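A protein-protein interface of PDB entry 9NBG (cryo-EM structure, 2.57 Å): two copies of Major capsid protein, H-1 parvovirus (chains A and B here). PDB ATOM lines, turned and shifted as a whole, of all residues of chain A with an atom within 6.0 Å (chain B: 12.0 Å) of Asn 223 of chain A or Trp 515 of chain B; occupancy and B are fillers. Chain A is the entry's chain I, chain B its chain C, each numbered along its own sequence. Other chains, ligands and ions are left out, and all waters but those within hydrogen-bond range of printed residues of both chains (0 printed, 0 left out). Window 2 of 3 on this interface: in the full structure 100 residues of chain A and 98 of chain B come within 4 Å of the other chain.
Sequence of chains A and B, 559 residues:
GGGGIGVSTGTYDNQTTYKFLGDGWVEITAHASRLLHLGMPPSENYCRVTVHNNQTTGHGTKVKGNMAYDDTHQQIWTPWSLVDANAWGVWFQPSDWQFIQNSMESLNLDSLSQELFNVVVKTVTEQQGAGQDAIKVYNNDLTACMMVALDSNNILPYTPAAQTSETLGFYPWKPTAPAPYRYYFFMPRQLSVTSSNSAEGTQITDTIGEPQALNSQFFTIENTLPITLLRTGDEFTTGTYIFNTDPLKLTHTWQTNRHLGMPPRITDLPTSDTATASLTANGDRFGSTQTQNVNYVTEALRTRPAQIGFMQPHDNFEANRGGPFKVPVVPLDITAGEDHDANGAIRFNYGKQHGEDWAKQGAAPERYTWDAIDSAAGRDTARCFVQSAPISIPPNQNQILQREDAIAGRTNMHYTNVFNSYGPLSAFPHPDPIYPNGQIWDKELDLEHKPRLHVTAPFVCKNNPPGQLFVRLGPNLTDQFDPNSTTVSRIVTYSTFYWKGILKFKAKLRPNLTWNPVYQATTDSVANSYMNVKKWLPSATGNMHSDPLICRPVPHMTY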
ATOM      1  N   PHE A 218      23.957   8.452  -7.143  1.00  0.00           N
ATOM      2  CA  PHE A 218      22.903   7.623  -7.780  1.00  0.00           C
ATOM      3  C   PHE A 218      23.510   6.293  -8.230  1.00  0.00           C
ATOM      4  O   PHE A 218      24.454   6.308  -9.039  1.00  0.00           O
ATOM      5  CB  PHE A 218      22.251   8.372  -8.945  1.00  0.00           C
ATOM      6  CG  PHE A 218      21.282   7.551  -9.755  1.00  0.00           C
ATOM      7  CD1 PHE A 218      20.203   6.930  -9.152  1.00  0.00           C
ATOM      8  CD2 PHE A 218      21.441   7.412 -11.123  1.00  0.00           C
ATOM      9  CE1 PHE A 218      19.310   6.176  -9.898  1.00  0.00           C
ATOM     10  CE2 PHE A 218      20.545   6.663 -11.870  1.00  0.00           C
ATOM     11  CZ  PHE A 218      19.481   6.045 -11.254  1.00  0.00           C
ATOM     12  N   PHE A 219      22.975   5.183  -7.723  1.00  0.00           N
ATOM     13  CA  PHE A 219      23.518   3.846  -8.070  1.00  0.00           C
ATOM     14  C   PHE A 219      22.454   3.038  -8.813  1.00  0.00           C
ATOM     15  O   PHE A 219      21.261   3.193  -8.498  1.00  0.00           O
ATOM     16  CB  PHE A 219      23.950   3.105  -6.805  1.00  0.00           C
ATOM     17  CG  PHE A 219      25.000   3.808  -5.984  1.00  0.00           C
ATOM     18  CD1 PHE A 219      26.252   4.077  -6.513  1.00  0.00           C
ATOM     19  CD2 PHE A 219      24.734   4.201  -4.683  1.00  0.00           C
ATOM     20  CE1 PHE A 219      27.216   4.723  -5.756  1.00  0.00           C
ATOM     21  CE2 PHE A 219      25.700   4.848  -3.927  1.00  0.00           C
ATOM     22  CZ  PHE A 219      26.938   5.106  -4.464  1.00  0.00           C
ATOM     23  N   THR A 220      22.878   2.190  -9.750  1.00  0.00           N
ATOM     24  CA  THR A 220      21.926   1.297 -10.456  1.00  0.00           C
ATOM     25  C   THR A 220      22.439  -0.139 -10.333  1.00  0.00           C
ATOM     26  O   THR A 220      23.647  -0.350 -10.544  1.00  0.00           O
ATOM     27  CB  THR A 220      21.774   1.680 -11.929  1.00  0.00           C
ATOM     28  OG1 THR A 220      23.032   1.441 -12.556  1.00  0.00           O
ATOM     29  CG2 THR A 220      21.358   3.120 -12.129  1.00  0.00           C
ATOM     30  N   ILE A 221      21.553  -1.080 -10.007  1.00  0.00           N
ATOM     31  CA  ILE A 221      21.976  -2.496  -9.824  1.00  0.00           C
ATOM     32  C   ILE A 221      22.724  -2.929 -11.086  1.00  0.00           C
ATOM     33  O   ILE A 221      23.777  -3.577 -10.951  1.00  0.00           O
ATOM     34  CB  ILE A 221      20.747  -3.388  -9.566  1.00  0.00           C
ATOM     35  CG1 ILE A 221      19.843  -2.811  -8.472  1.00  0.00           C
ATOM     36  CG2 ILE A 221      21.165  -4.816  -9.260  1.00  0.00           C
ATOM     37  CD1 ILE A 221      20.307  -3.114  -7.070  1.00  0.00           C
ATOM     38  N   GLU A 222      22.232  -2.522 -12.256  1.00  0.00           N
ATOM     39  CA  GLU A 222      22.830  -2.963 -13.544  1.00  0.00           C
ATOM     40  C   GLU A 222      24.267  -2.461 -13.700  1.00  0.00           C
ATOM     41  O   GLU A 222      25.105  -3.249 -14.174  1.00  0.00           O
ATOM     42  CB  GLU A 222      21.988  -2.450 -14.711  1.00  0.00           C
ATOM     43  CG  GLU A 222      20.645  -3.145 -14.853  1.00  0.00           C
ATOM     44  CD  GLU A 222      19.552  -2.649 -13.922  1.00  0.00           C
ATOM     45  OE1 GLU A 222      19.839  -1.758 -13.100  1.00  0.00           O
ATOM     46  OE2 GLU A 222      18.417  -3.147 -14.035  1.00  0.00           O
ATOM     47  N   ASN A 223      24.547  -1.212 -13.331  1.00  0.00           N
ATOM     48  CA  ASN A 223      25.903  -0.652 -13.588  1.00  0.00           C
ATOM     49  C   ASN A 223      26.842  -0.929 -12.413  1.00  0.00           C
ATOM     50  O   ASN A 223      27.977  -0.423 -12.449  1.00  0.00           O
ATOM     51  CB  ASN A 223      25.847   0.848 -13.888  1.00  0.00           C
ATOM     52  CG  ASN A 223      25.111   1.164 -15.171  1.00  0.00           C
ATOM     53  OD1 ASN A 223      25.515   0.731 -16.246  1.00  0.00           O
ATOM     54  ND2 ASN A 223      24.033   1.924 -15.066  1.00  0.00           N
ATOM     55  N   THR A 224      26.415  -1.753 -11.452  1.00  0.00           N
ATOM     56  CA  THR A 224      27.245  -1.983 -10.241  1.00  0.00           C
ATOM     57  C   THR A 224      27.392  -3.475  -9.931  1.00  0.00           C
ATOM     58  O   THR A 224      28.464  -3.851  -9.425  1.00  0.00           O
ATOM     59  CB  THR A 224      26.642  -1.276  -9.024  1.00  0.00           C
ATOM     60  OG1 THR A 224      25.300  -1.741  -8.875  1.00  0.00           O
ATOM     61  CG2 THR A 224      26.652   0.233  -9.147  1.00  0.00           C
ATOM     62  N   LEU A 225      26.373  -4.289 -10.214  1.00  0.00           N
ATOM     63  CA  LEU A 225      26.434  -5.719  -9.804  1.00  0.00           C
ATOM     64  C   LEU A 225      26.384  -6.652 -11.011  1.00  0.00           C
ATOM     65  O   LEU A 225      25.729  -6.293 -12.005  1.00  0.00           O
ATOM     66  CB  LEU A 225      25.231  -6.019  -8.911  1.00  0.00           C
ATOM     67  CG  LEU A 225      25.077  -5.148  -7.669  1.00  0.00           C
ATOM     68  CD1 LEU A 225      24.010  -5.731  -6.756  1.00  0.00           C
ATOM     69  CD2 LEU A 225      26.401  -5.032  -6.937  1.00  0.00           C
ATOM     70  N   ARG B 510      40.684   6.225  -6.009  1.00  0.00           N
ATOM     71  CA  ARG B 510      39.267   6.080  -5.583  1.00  0.00           C
ATOM     72  C   ARG B 510      38.502   5.235  -6.602  1.00  0.00           C
ATOM     73  O   ARG B 510      38.865   5.270  -7.793  1.00  0.00           O
ATOM     74  CB  ARG B 510      38.608   7.455  -5.440  1.00  0.00           C
ATOM     75  CG  ARG B 510      38.307   8.153  -6.757  1.00  0.00           C
ATOM     76  CD  ARG B 510      37.737   9.540  -6.534  1.00  0.00           C
ATOM     77  NE  ARG B 510      37.320  10.192  -7.767  1.00  0.00           N
ATOM     78  CZ  ARG B 510      36.345   9.761  -8.558  1.00  0.00           C
ATOM     79  NH1 ARG B 510      35.495   8.846  -8.130  1.00  0.00           N
ATOM     80  NH2 ARG B 510      36.214  10.262  -9.775  1.00  0.00           N
ATOM     81  N   PRO B 511      37.462   4.456  -6.210  1.00  0.00           N
ATOM     82  CA  PRO B 511      36.655   3.724  -7.184  1.00  0.00           C
ATOM     83  C   PRO B 511      35.514   4.601  -7.715  1.00  0.00           C
ATOM     84  O   PRO B 511      35.072   5.482  -7.003  1.00  0.00           O
ATOM     85  CB  PRO B 511      36.082   2.573  -6.353  1.00  0.00           C
ATOM     86  CG  PRO B 511      35.893   3.174  -4.980  1.00  0.00           C
ATOM     87  CD  PRO B 511      37.016   4.180  -4.834  1.00  0.00           C
ATOM     88  N   ASN B 512      35.078   4.353  -8.953  1.00  0.00           N
ATOM     89  CA  ASN B 512      33.936   5.114  -9.521  1.00  0.00           C
ATOM     90  C   ASN B 512      32.781   4.139  -9.760  1.00  0.00           C
ATOM     91  O   ASN B 512      32.921   3.275 -10.644  1.00  0.00           O
ATOM     92  CB  ASN B 512      34.314   5.855 -10.803  1.00  0.00           C
ATOM     93  CG  ASN B 512      33.160   6.645 -11.380  1.00  0.00           C
ATOM     94  OD1 ASN B 512      32.614   7.525 -10.719  1.00  0.00           O
ATOM     95  ND2 ASN B 512      32.779   6.336 -12.609  1.00  0.00           N
ATOM     96  N   LEU B 513      31.704   4.244  -8.983  1.00  0.00           N
ATOM     97  CA  LEU B 513      30.595   3.259  -9.104  1.00  0.00           C
ATOM     98  C   LEU B 513      29.249   3.989  -9.107  1.00  0.00           C
ATOM     99  O   LEU B 513      28.224   3.325  -8.881  1.00  0.00           O
ATOM    100  CB  LEU B 513      30.680   2.282  -7.928  1.00  0.00           C
ATOM    101  CG  LEU B 513      31.868   1.322  -7.951  1.00  0.00           C
ATOM    102  CD1 LEU B 513      31.851   0.414  -6.732  1.00  0.00           C
ATOM    103  CD2 LEU B 513      31.864   0.491  -9.224  1.00  0.00           C
ATOM    104  N   THR B 514      29.259   5.299  -9.353  1.00  0.00           N
ATOM    105  CA  THR B 514      28.001   6.088  -9.326  1.00  0.00           C
ATOM    106  C   THR B 514      27.639   6.536 -10.741  1.00  0.00           C
ATOM    107  O   THR B 514      28.544   6.981 -11.466  1.00  0.00           O
ATOM    108  CB  THR B 514      28.123   7.301  -8.396  1.00  0.00           C
ATOM    109  OG1 THR B 514      29.089   8.188  -8.960  1.00  0.00           O
ATOM    110  CG2 THR B 514      28.529   6.923  -6.989  1.00  0.00           C
ATOM    111  N   TRP B 515      26.366   6.437 -11.125  1.00  0.00           N
ATOM    112  CA  TRP B 515      25.951   6.930 -12.465  1.00  0.00           C
ATOM    113  C   TRP B 515      26.183   8.440 -12.551  1.00  0.00           C
ATOM    114  O   TRP B 515      26.817   8.883 -13.525  1.00  0.00           O
ATOM    115  CB  TRP B 515      24.490   6.569 -12.753  1.00  0.00           C
ATOM    116  CG  TRP B 515      23.952   7.180 -14.011  1.00  0.00           C
ATOM    117  CD1 TRP B 515      23.545   8.468 -14.195  1.00  0.00           C
ATOM    118  CD2 TRP B 515      23.797   6.527 -15.282  1.00  0.00           C
ATOM    119  NE1 TRP B 515      23.130   8.659 -15.485  1.00  0.00           N
ATOM    120  CE2 TRP B 515      23.274   7.485 -16.176  1.00  0.00           C
ATOM    121  CE3 TRP B 515      24.039   5.231 -15.751  1.00  0.00           C
ATOM    122  CZ2 TRP B 515      22.992   7.185 -17.507  1.00  0.00           C
ATOM    123  CZ3 TRP B 515      23.760   4.936 -17.065  1.00  0.00           C
ATOM    124  CH2 TRP B 515      23.243   5.899 -17.929  1.00  0.00           C
ATOM    125  N   ASN B 516      25.691   9.192 -11.566  1.00  0.00           N
ATOM    126  CA  ASN B 516      25.803  10.671 -11.613  1.00  0.00           C
ATOM    127  C   ASN B 516      27.271  11.095 -11.603  1.00  0.00           C
ATOM    128  O   ASN B 516      28.081  10.406 -10.958  1.00  0.00           O
ATOM    129  CB  ASN B 516      25.059  11.336 -10.454  1.00  0.00           C
ATOM    130  CG  ASN B 516      25.387  10.734  -9.105  1.00  0.00           C
ATOM    131  OD1 ASN B 516      26.101   9.738  -9.017  1.00  0.00           O
ATOM    132  ND2 ASN B 516      24.854  11.321  -8.047  1.00  0.00           N
ATOM    133  N   PRO B 517      27.694  12.152 -12.338  1.00  0.00           N
ATOM    134  CA  PRO B 517      29.075  12.624 -12.250  1.00  0.00           C
ATOM    135  C   PRO B 517      29.380  13.025 -10.802  1.00  0.00           C
ATOM    136  O   PRO B 517      28.467  13.428 -10.109  1.00  0.00           O
ATOM    137  CB  PRO B 517      29.113  13.851 -13.166  1.00  0.00           C
ATOM    138  CG  PRO B 517      27.996  13.600 -14.150  1.00  0.00           C
ATOM    139  CD  PRO B 517      26.923  12.931 -13.321  1.00  0.00           C
ATOM    140  N   VAL B 518      30.642  12.923 -10.383  1.00  0.00           N
ATOM    141  CA  VAL B 518      30.990  13.198  -8.958  1.00  0.00           C
ATOM    142  C   VAL B 518      31.559  14.613  -8.827  1.00  0.00           C
ATOM    143  O   VAL B 518      32.179  15.090  -9.794  1.00  0.00           O
ATOM    144  CB  VAL B 518      31.981  12.152  -8.420  1.00  0.00           C
ATOM    145  CG1 VAL B 518      32.079  12.209  -6.906  1.00  0.00           C
ATOM    146  CG2 VAL B 518      31.612  10.747  -8.874  1.00  0.00           C
ATOM    147  N   TYR B 519      31.360  15.256  -7.673  1.00  0.00           N
ATOM    148  CA  TYR B 519      31.924  16.610  -7.438  1.00  0.00           C
ATOM    149  C   TYR B 519      33.449  16.520  -7.372  1.00  0.00           C
ATOM    150  O   TYR B 519      33.968  15.672  -6.622  1.00  0.00           O
ATOM    151  CB  TYR B 519      31.375  17.212  -6.145  1.00  0.00           C
ATOM    152  CG  TYR B 519      31.992  18.531  -5.760  1.00  0.00           C
ATOM    153  CD1 TYR B 519      31.873  19.642  -6.578  1.00  0.00           C
ATOM    154  CD2 TYR B 519      32.707  18.669  -4.582  1.00  0.00           C
ATOM    155  CE1 TYR B 519      32.439  20.857  -6.232  1.00  0.00           C
ATOM    156  CE2 TYR B 519      33.280  19.877  -4.221  1.00  0.00           C
ATOM    157  CZ  TYR B 519      33.146  20.976  -5.049  1.00  0.00           C
ATOM    158  OH  TYR B 519      33.711  22.176  -4.699  1.00  0.00           O
ATOM    159  N   GLN B 520      34.143  17.371  -8.128  1.00  0.00           N
ATOM    160  CA  GLN B 520      35.629  17.363  -8.138  1.00  0.00           C
ATOM    161  C   GLN B 520      36.136  18.771  -7.831  1.00  0.00           C
ATOM    162  O   GLN B 520      35.424  19.737  -8.162  1.00  0.00           O
ATOM    163  CB  GLN B 520      36.147  16.896  -9.498  1.00  0.00           C
ATOM    164  CG  GLN B 520      35.623  15.534  -9.923  1.00  0.00           C
ATOM    165  CD  GLN B 520      36.034  14.443  -8.969  1.00  0.00           C
ATOM    166  OE1 GLN B 520      37.218  14.205  -8.743  1.00  0.00           O
ATOM    167  NE2 GLN B 520      35.052  13.766  -8.399  1.00  0.00           N
ATOM    168  N   VAL B 554      34.791  13.957  -2.875  1.00  0.00           N
ATOM    169  CA  VAL B 554      33.925  12.823  -3.309  1.00  0.00           C
ATOM    170  C   VAL B 554      33.164  12.282  -2.098  1.00  0.00           C
ATOM    171  O   VAL B 554      33.802  12.059  -1.056  1.00  0.00           O
ATOM    172  CB  VAL B 554      34.765  11.725  -3.989  1.00  0.00           C
ATOM    173  CG1 VAL B 554      33.940  10.491  -4.317  1.00  0.00           C
ATOM    174  CG2 VAL B 554      35.476  12.245  -5.227  1.00  0.00           C
ATOM    175  N   PRO B 555      31.833  12.081  -2.180  1.00  0.00           N
ATOM    176  CA  PRO B 555      31.071  11.503  -1.075  1.00  0.00           C
ATOM    177  C   PRO B 555      31.146   9.971  -1.029  1.00  0.00           C
ATOM    178  O   PRO B 555      31.318   9.370  -2.072  1.00  0.00           O
ATOM    179  CB  PRO B 555      29.636  11.926  -1.414  1.00  0.00           C
ATOM    180  CG  PRO B 555      29.609  11.969  -2.924  1.00  0.00           C
ATOM    181  CD  PRO B 555      30.993  12.435  -3.327  1.00  0.00           C
ATOM    182  N   MET B 557      29.172   6.348   0.798  1.00  0.00           N
ATOM    183  CA  MET B 557      27.974   5.877   1.545  1.00  0.00           C
ATOM    184  C   MET B 557      28.397   5.473   2.960  1.00  0.00           C
ATOM    185  O   MET B 557      29.372   4.711   3.086  1.00  0.00           O
ATOM    186  CB  MET B 557      27.335   4.674   0.848  1.00  0.00           C
ATOM    187  CG  MET B 557      25.933   4.372   1.331  1.00  0.00           C
ATOM    188  SD  MET B 557      24.813   5.758   1.021  1.00  0.00           S
ATOM    189  CE  MET B 557      24.356   5.438  -0.682  1.00  0.00           C
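The backbone carbonyl oxygen (O) of Phe 218 of chain A is in hydrogen-bond range of the backbone NH (N) of Trp 515 of chain B, at 2.8 Å.
OD1 of Asn 516 of chain B sits at hydrogen-bond distance from N of Phe 218 of chain A (3.1 Å).
OG1 of Thr 514 of chain B sits at hydrogen-bond distance from O of Asn 516 of chain B (3.2 Å).
The side-chain hydroxyl (OG1) of Thr 220 of chain A is in hydrogen-bond range of the side-chain amide nitrogen (ND2) of Asn 223 of chain A (2.7 Å).
O of Thr 220 of chain A is in hydrogen-bond range of OG1 of Thr 224 of chain A (2.7 Å).
The backbone carbonyl oxygen (O) of Ile 221 of chain A sits at hydrogen-bond distance from the side-chain hydroxyl (OG1) of Thr 224 of chain A, 3.2 Å away.
Of chain B, only Leu 513, Thr 514 and Met 557 come within 4 Å of Phe 219 of chain A.
No residue of chain B comes within 4 Å of Thr 220 of chain A.
Glu 222 of chain A touches none of the printed residues of chain B.
Printed residues of chain A within 4 Å of Asn 516 of chain B: Phe 218 (3.1 Å).
Printed residues of chain A within 4 Å of Met 557 of chain B: Phe 219 (3.6 Å).
Printed residues of chain A within 4 Å of Leu 513 of chain B: Phe 219 and Thr 224.
Of the printed residues of chain A, Thr 514 of chain B touches Phe 218 and Phe 219.
Pro 555 of chain B touches none of the printed residues of chain A.
The nearest printed residue of chain A that does not touch Met 557 of chain B is Phe 218 of chain A (7.1 Å).
No position is printed for both chains.
O of Phe 218 of chain A touches CA of Thr 514 of chain B (3.6 Å).
Phe 219 of chain A touches Leu 513 of chain B.
Thr 514 of chain B touches Phe 219 of chain A.
Met 557 of chain B touches Phe 219 of chain A (CE to CE2, 3.6 Å).
Trp 515 of chain B touches Asn 223 of chain A (CE3 to ND2, 3.4 Å).
Leu 513 of chain B touches Thr 224 of chain A (O to CG2, 3.5 Å).
Of the 14 printed residues of chain B, 5 touch a printed residue of chain A.
Of the 8 printed residues of chain A, 4 touch a printed residue of chain B.
Printed residues of chain A that touch a printed residue of chain B: Phe 218, Phe 219, Asn 223 and Thr 224.
Among the printed residues, 8 pairs touch across the chains.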
